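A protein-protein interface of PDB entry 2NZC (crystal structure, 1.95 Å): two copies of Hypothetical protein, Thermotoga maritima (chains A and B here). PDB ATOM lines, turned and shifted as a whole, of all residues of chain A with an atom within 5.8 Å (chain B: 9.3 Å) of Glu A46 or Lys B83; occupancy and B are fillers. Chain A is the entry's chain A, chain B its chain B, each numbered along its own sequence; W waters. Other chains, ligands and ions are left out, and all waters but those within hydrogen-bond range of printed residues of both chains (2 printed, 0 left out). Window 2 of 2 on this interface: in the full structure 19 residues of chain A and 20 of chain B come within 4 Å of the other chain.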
ATOM      1  N   VAL A  43      16.354 -13.456  29.109  1.00  0.00           N
ATOM      2  CA  VAL A  43      15.522 -13.652  27.944  1.00  0.00           C
ATOM      3  C   VAL A  43      14.448 -14.654  28.335  1.00  0.00           C
ATOM      4  O   VAL A  43      14.600 -15.853  28.132  1.00  0.00           O
ATOM      5  CB  VAL A  43      16.350 -14.158  26.744  1.00  0.00           C
ATOM      6  CG1 VAL A  43      15.484 -14.203  25.483  1.00  0.00           C
ATOM      7  CG2 VAL A  43      17.566 -13.262  26.549  1.00  0.00           C
ATOM      8  N   ARG A  44      13.370 -14.166  28.938  1.00  0.00           N
ATOM      9  CA  ARG A  44      12.374 -15.079  29.497  1.00  0.00           C
ATOM     10  C   ARG A  44      11.683 -15.916  28.450  1.00  0.00           C
ATOM     11  O   ARG A  44      11.341 -17.089  28.700  1.00  0.00           O
ATOM     12  CB  ARG A  44      11.383 -14.347  30.405  1.00  0.00           C
ATOM     13  CG  ARG A  44      12.156 -13.649  31.535  1.00  0.00           C
ATOM     14  CD  ARG A  44      11.339 -13.415  32.792  1.00  0.00           C
ATOM     15  NE  ARG A  44      12.256 -13.353  33.936  1.00  0.00           N
ATOM     16  CZ  ARG A  44      12.959 -12.275  34.299  1.00  0.00           C
ATOM     17  NH1 ARG A  44      12.850 -11.125  33.633  1.00  0.00           N
ATOM     18  NH2 ARG A  44      13.763 -12.350  35.352  1.00  0.00           N
ATOM     19  N   GLU A  45      11.499 -15.354  27.263  1.00  0.00           N
ATOM     20  CA  GLU A  45      10.788 -16.115  26.247  1.00  0.00           C
ATOM     21  C   GLU A  45      11.622 -17.293  25.732  1.00  0.00           C
ATOM     22  O   GLU A  45      11.102 -18.153  25.040  1.00  0.00           O
ATOM     23  CB  GLU A  45      10.257 -15.223  25.123  1.00  0.00           C
ATOM     24  CG  GLU A  45      11.235 -14.910  24.023  1.00  0.00           C
ATOM     25  CD  GLU A  45      10.671 -13.878  23.059  1.00  0.00           C
ATOM     26  OE1 GLU A  45      10.319 -14.267  21.935  1.00  0.00           O
ATOM     27  OE2 GLU A  45      10.574 -12.685  23.437  1.00  0.00           O
ATOM     28  N   GLU A  46      12.891 -17.347  26.111  1.00  0.00           N
ATOM     29  CA  GLU A  46      13.774 -18.460  25.747  1.00  0.00           C
ATOM     30  C   GLU A  46      14.285 -19.265  26.947  1.00  0.00           C
ATOM     31  O   GLU A  46      15.064 -20.201  26.771  1.00  0.00           O
ATOM     32  CB  GLU A  46      14.967 -17.963  24.921  1.00  0.00           C
ATOM     33  CG  GLU A  46      14.601 -17.348  23.559  1.00  0.00           C
ATOM     34  CD  GLU A  46      13.674 -18.191  22.726  1.00  0.00           C
ATOM     35  OE1 GLU A  46      13.837 -19.426  22.691  1.00  0.00           O
ATOM     36  OE2 GLU A  46      12.771 -17.609  22.088  1.00  0.00           O
ATOM     37  N   ASN A  47      13.841 -18.884  28.147  1.00  0.00           N
ATOM     38  CA  ASN A  47      14.346 -19.418  29.427  1.00  0.00           C
ATOM     39  C   ASN A  47      15.845 -19.450  29.513  1.00  0.00           C
ATOM     40  O   ASN A  47      16.455 -20.497  29.733  1.00  0.00           O
ATOM     41  CB  ASN A  47      13.710 -20.764  29.776  1.00  0.00           C
ATOM     42  CG  ASN A  47      12.210 -20.640  29.994  1.00  0.00           C
ATOM     43  OD1 ASN A  47      11.428 -21.397  29.439  1.00  0.00           O
ATOM     44  ND2 ASN A  47      11.806 -19.631  30.774  1.00  0.00           N
ATOM     45  N   MET A  48      16.430 -18.272  29.309  1.00  0.00           N
ATOM     46  CA  MET A  48      17.847 -18.123  29.262  1.00  0.00           C
ATOM     47  C   MET A  48      18.185 -16.742  29.795  1.00  0.00           C
ATOM     48  O   MET A  48      17.311 -15.896  29.925  1.00  0.00           O
ATOM     49  CB  MET A  48      18.331 -18.254  27.821  1.00  0.00           C
ATOM     50  CG  MET A  48      17.872 -19.530  27.128  1.00  0.00           C
ATOM     51  SD  MET A  48      19.023 -19.878  25.640  1.00  0.00           S
ATOM     52  CE  MET A  48      20.636 -20.089  26.691  1.00  0.00           C
ATOM     53  N   ARG A  76      27.409 -21.282  28.040  1.00  0.00           N
ATOM     54  CA  ARG A  76      28.265 -21.078  26.886  1.00  0.00           C
ATOM     55  C   ARG A  76      28.998 -19.776  27.155  1.00  0.00           C
ATOM     56  O   ARG A  76      28.385 -18.800  27.626  1.00  0.00           O
ATOM     57  CB  ARG A  76      27.434 -20.946  25.616  1.00  0.00           C
ATOM     58  CG  ARG A  76      26.911 -22.251  25.050  1.00  0.00           C
ATOM     59  CD  ARG A  76      25.758 -21.967  24.096  1.00  0.00           C
ATOM     60  NE  ARG A  76      26.153 -21.128  22.966  1.00  0.00           N
ATOM     61  CZ  ARG A  76      25.365 -20.218  22.401  1.00  0.00           C
ATOM     62  NH1 ARG A  76      24.142 -20.014  22.873  1.00  0.00           N
ATOM     63  NH2 ARG A  76      25.801 -19.514  21.366  1.00  0.00           N
ATOM     64  N   GLU B   4      10.527 -16.387  13.459  1.00  0.00           N
ATOM     65  CA  GLU B   4      11.497 -16.328  12.322  1.00  0.00           C
ATOM     66  C   GLU B   4      12.630 -15.365  12.714  1.00  0.00           C
ATOM     67  O   GLU B   4      13.726 -15.409  12.139  1.00  0.00           O
ATOM     68  CB  GLU B   4      10.785 -15.878  11.046  1.00  0.00           C
ATOM     69  CG  GLU B   4      11.294 -16.529   9.756  1.00  0.00           C
ATOM     70  CD  GLU B   4      10.176 -16.819   8.766  1.00  0.00           C
ATOM     71  OE1 GLU B   4       9.004 -16.530   9.094  1.00  0.00           O
ATOM     72  OE2 GLU B   4      10.452 -17.343   7.658  1.00  0.00           O
ATOM     73  N   LYS B   5      12.335 -14.502  13.691  1.00  0.00           N
ATOM     74  CA  LYS B   5      13.310 -13.641  14.338  1.00  0.00           C
ATOM     75  C   LYS B   5      13.960 -14.369  15.515  1.00  0.00           C
ATOM     76  O   LYS B   5      13.277 -15.053  16.289  1.00  0.00           O
ATOM     77  CB  LYS B   5      12.653 -12.369  14.865  1.00  0.00           C
ATOM     78  CG  LYS B   5      12.003 -11.493  13.805  1.00  0.00           C
ATOM     79  CD  LYS B   5      11.918 -10.092  14.369  1.00  0.00           C
ATOM     80  CE  LYS B   5      11.041  -9.182  13.537  1.00  0.00           C
ATOM     81  NZ  LYS B   5      11.080  -7.805  14.126  1.00  0.00           N
ATOM     82  N   ARG B   6      15.271 -14.201  15.645  1.00  0.00           N
ATOM     83  CA  ARG B   6      16.039 -14.867  16.686  1.00  0.00           C
ATOM     84  C   ARG B   6      16.862 -13.847  17.465  1.00  0.00           C
ATOM     85  O   ARG B   6      17.128 -12.755  16.956  1.00  0.00           O
ATOM     86  CB  ARG B   6      16.970 -15.901  16.057  1.00  0.00           C
ATOM     87  CG  ARG B   6      16.248 -17.099  15.435  1.00  0.00           C
ATOM     88  CD  ARG B   6      17.241 -18.144  14.933  1.00  0.00           C
ATOM     89  NE  ARG B   6      18.297 -18.382  15.915  1.00  0.00           N
ATOM     90  CZ  ARG B   6      19.410 -19.070  15.690  1.00  0.00           C
ATOM     91  NH1 ARG B   6      19.645 -19.629  14.502  1.00  0.00           N
ATOM     92  NH2 ARG B   6      20.287 -19.211  16.669  1.00  0.00           N
ATOM     93  N   PHE B   7      17.248 -14.203  18.697  1.00  0.00           N
ATOM     94  CA  PHE B   7      18.164 -13.371  19.519  1.00  0.00           C
ATOM     95  C   PHE B   7      19.632 -13.560  19.155  1.00  0.00           C
ATOM     96  O   PHE B   7      20.098 -14.700  18.935  1.00  0.00           O
ATOM     97  CB  PHE B   7      17.996 -13.660  21.015  1.00  0.00           C
ATOM     98  CG  PHE B   7      16.669 -13.246  21.558  1.00  0.00           C
ATOM     99  CD1 PHE B   7      15.570 -14.106  21.463  1.00  0.00           C
ATOM    100  CD2 PHE B   7      16.500 -12.014  22.153  1.00  0.00           C
ATOM    101  CE1 PHE B   7      14.315 -13.729  21.971  1.00  0.00           C
ATOM    102  CE2 PHE B   7      15.224 -11.631  22.669  1.00  0.00           C
ATOM    103  CZ  PHE B   7      14.157 -12.499  22.570  1.00  0.00           C
ATOM    104  N   TYR B   8      20.357 -12.441  19.093  1.00  0.00           N
ATOM    105  CA  TYR B   8      21.777 -12.450  18.808  1.00  0.00           C
ATOM    106  C   TYR B   8      22.419 -11.513  19.781  1.00  0.00           C
ATOM    107  O   TYR B   8      21.796 -10.569  20.239  1.00  0.00           O
ATOM    108  CB  TYR B   8      22.038 -11.955  17.383  1.00  0.00           C
ATOM    109  CG  TYR B   8      21.435 -12.856  16.347  1.00  0.00           C
ATOM    110  CD1 TYR B   8      22.075 -14.032  15.988  1.00  0.00           C
ATOM    111  CD2 TYR B   8      20.194 -12.566  15.775  1.00  0.00           C
ATOM    112  CE1 TYR B   8      21.523 -14.893  15.059  1.00  0.00           C
ATOM    113  CE2 TYR B   8      19.629 -13.416  14.822  1.00  0.00           C
ATOM    114  CZ  TYR B   8      20.299 -14.587  14.489  1.00  0.00           C
ATOM    115  OH  TYR B   8      19.791 -15.440  13.557  1.00  0.00           O
ATOM    116  N   ILE B   9      23.681 -11.784  20.087  1.00  0.00           N
ATOM    117  CA  ILE B   9      24.466 -10.962  20.965  1.00  0.00           C
ATOM    118  C   ILE B   9      25.619 -10.460  20.108  1.00  0.00           C
ATOM    119  O   ILE B   9      26.243 -11.267  19.429  1.00  0.00           O
ATOM    120  CB  ILE B   9      25.097 -11.839  22.070  1.00  0.00           C
ATOM    121  CG1 ILE B   9      24.057 -12.724  22.763  1.00  0.00           C
ATOM    122  CG2 ILE B   9      25.775 -10.967  23.088  1.00  0.00           C
ATOM    123  CD1 ILE B   9      23.115 -11.951  23.561  1.00  0.00           C
ATOM    124  N   LEU B  55      20.014  -8.112  20.055  1.00  0.00           N
ATOM    125  CA  LEU B  55      19.041  -7.878  19.000  1.00  0.00           C
ATOM    126  C   LEU B  55      18.108  -9.075  18.901  1.00  0.00           C
ATOM    127  O   LEU B  55      18.482 -10.164  19.286  1.00  0.00           O
ATOM    128  CB  LEU B  55      19.723  -7.736  17.625  1.00  0.00           C
ATOM    129  CG  LEU B  55      20.624  -6.515  17.416  1.00  0.00           C
ATOM    130  CD1 LEU B  55      22.016  -6.893  17.762  1.00  0.00           C
ATOM    131  CD2 LEU B  55      20.535  -6.105  15.972  1.00  0.00           C
ATOM    132  N   LYS B  56      16.886  -8.851  18.449  1.00  0.00           N
ATOM    133  CA  LYS B  56      16.026  -9.947  18.043  1.00  0.00           C
ATOM    134  C   LYS B  56      15.660  -9.611  16.627  1.00  0.00           C
ATOM    135  O   LYS B  56      14.994  -8.596  16.373  1.00  0.00           O
ATOM    136  CB  LYS B  56      14.800 -10.074  18.930  1.00  0.00           C
ATOM    137  CG  LYS B  56      14.037 -11.348  18.653  1.00  0.00           C
ATOM    138  CD  LYS B  56      12.761 -11.392  19.420  1.00  0.00           C
ATOM    139  CE  LYS B  56      11.929 -12.549  18.943  1.00  0.00           C
ATOM    140  NZ  LYS B  56      10.641 -12.604  19.686  1.00  0.00           N
ATOM    141  N   VAL B  80      27.124 -13.771  18.250  1.00  0.00           N
ATOM    142  CA  VAL B  80      26.835 -15.063  18.882  1.00  0.00           C
ATOM    143  C   VAL B  80      25.312 -15.252  18.877  1.00  0.00           C
ATOM    144  O   VAL B  80      24.591 -14.351  19.343  1.00  0.00           O
ATOM    145  CB  VAL B  80      27.261 -14.982  20.398  1.00  0.00           C
ATOM    146  CG1 VAL B  80      27.011 -16.287  21.126  1.00  0.00           C
ATOM    147  CG2 VAL B  80      28.733 -14.607  20.536  1.00  0.00           C
ATOM    148  N   PRO B  81      24.805 -16.407  18.384  1.00  0.00           N
ATOM    149  CA  PRO B  81      23.361 -16.574  18.579  1.00  0.00           C
ATOM    150  C   PRO B  81      23.040 -16.962  20.021  1.00  0.00           C
ATOM    151  O   PRO B  81      23.851 -17.628  20.658  1.00  0.00           O
ATOM    152  CB  PRO B  81      22.994 -17.703  17.617  1.00  0.00           C
ATOM    153  CG  PRO B  81      24.259 -18.529  17.481  1.00  0.00           C
ATOM    154  CD  PRO B  81      25.420 -17.555  17.684  1.00  0.00           C
ATOM    155  N   LEU B  82      21.886 -16.538  20.540  1.00  0.00           N
ATOM    156  CA  LEU B  82      21.463 -16.949  21.876  1.00  0.00           C
ATOM    157  C   LEU B  82      21.268 -18.460  21.932  1.00  0.00           C
ATOM    158  O   LEU B  82      21.655 -19.105  22.905  1.00  0.00           O
ATOM    159  CB  LEU B  82      20.154 -16.269  22.239  1.00  0.00           C
ATOM    160  CG  LEU B  82      19.605 -16.538  23.625  1.00  0.00           C
ATOM    161  CD1 LEU B  82      20.487 -15.857  24.683  1.00  0.00           C
ATOM    162  CD2 LEU B  82      18.158 -16.068  23.715  1.00  0.00           C
ATOM    163  N   LYS B  83      20.662 -19.012  20.886  1.00  0.00           N
ATOM    164  CA  LYS B  83      20.416 -20.437  20.795  1.00  0.00           C
ATOM    165  C   LYS B  83      21.276 -21.022  19.675  1.00  0.00           C
ATOM    166  O   LYS B  83      21.297 -20.493  18.565  1.00  0.00           O
ATOM    167  CB  LYS B  83      18.927 -20.694  20.570  1.00  0.00           C
ATOM    168  CG  LYS B  83      18.104 -20.241  21.773  1.00  0.00           C
ATOM    169  CD  LYS B  83      16.619 -20.419  21.565  1.00  0.00           C
ATOM    170  CE  LYS B  83      16.193 -21.861  21.634  1.00  0.00           C
ATOM    171  NZ  LYS B  83      14.744 -21.956  21.275  1.00  0.00           N
ATOM    172  N   ARG B  84      22.007 -22.084  19.997  1.00  0.00           N
ATOM    173  CA  ARG B  84      23.015 -22.647  19.099  1.00  0.00           C
ATOM    174  C   ARG B  84      22.448 -23.199  17.812  1.00  0.00           C
ATOM    175  O   ARG B  84      21.304 -23.645  17.774  1.00  0.00           O
HETATM  176  O   HOH W   1      22.530 -21.185  24.431  1.00  0.00           O
HETATM  177  O   HOH W   2       9.881 -10.979  21.516  1.00  0.00           O
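Along chain A the printed residues that touch a printed residue of chain B span positions 43 to 76. Of the 13 printed residues of chain B, 6 touch a printed residue of chain A. Hydrophobic or aromatic side chains of chain B within 4 Å of the printed part of chain A: Phe B7, Val B80 and Leu B82.
Of the printed residues of chain B, Val A43 touches Phe B7 and Leu B82. Of chain B, only Phe B7, Leu B82 and Lys B83 come within 4 Å of Glu A46. No residue of chain B comes within 4 Å of Asn A47. Printed residues of chain B within 4 Å of Arg A76: Val B80, Pro B81 and Leu B82. Arg B6 touches none of the printed residues of chain A. Leu B55 touches none of the printed residues of chain A. Of the printed residues of chain A, Pro B81 touches Arg A76 (2.8 Å). Of the printed residues of chain A, Lys B83 touches Glu A46 (3.0 Å) and Met A48 (3.99 Å). The nearest printed residue of chain B that does not touch Met A48 is Arg B84 (6.8 Å).
The side-chain carboxylate of Glu A45 is in salt-bridge range of the side-chain amino group of Lys B56 (2.8 Å). The side-chain amino group of Lys B83 is in salt-bridge range of the side-chain carboxylate of Glu A46 (3.0 Å). The guanidinium group (NH2) of Arg A76 is in hydrogen-bond range of the backbone carbonyl oxygen (O) of Pro B81 (2.8 Å). NH1 of Arg A76 lies within hydrogen-bond range of O of Leu B82 (2.6 Å).
O of Met A48 is in hydrogen-bond range of N of Val A43 (2.7 Å). The guanidinium group (NH2) of Arg B6 is in hydrogen-bond range of the backbone carbonyl oxygen (O) of Lys B83 (2.5 Å). O of Phe B7 sits at hydrogen-bond distance from N of Leu B82. N of Ile B9 lies within hydrogen-bond range of O of Val B80, at 2.8 Å.
Water W1 lies within hydrogen-bond range of the guanidinium group (NH1) of Arg A76 (2.5 Å) and the backbone carbonyl oxygen (O) of Leu B82 (2.7 Å). Water W2 bridges NZ of Lys B56 and OE2 of Glu A45.
Among the printed residues, pairs that only touch across the chains: Arg A76 with Val B80, Val A43 with Phe B7, Glu A45 with Phe B7, Val A43 with Leu B82, Glu A46 with Leu B82, Met A48 with Leu B82, Glu A46 with Phe B7 and Met A48 with Lys B83.
No position is printed for both chains. Of the 12 pairs that touch across the chains among the printed residues, none has its exchanged pair printed and touching as well.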
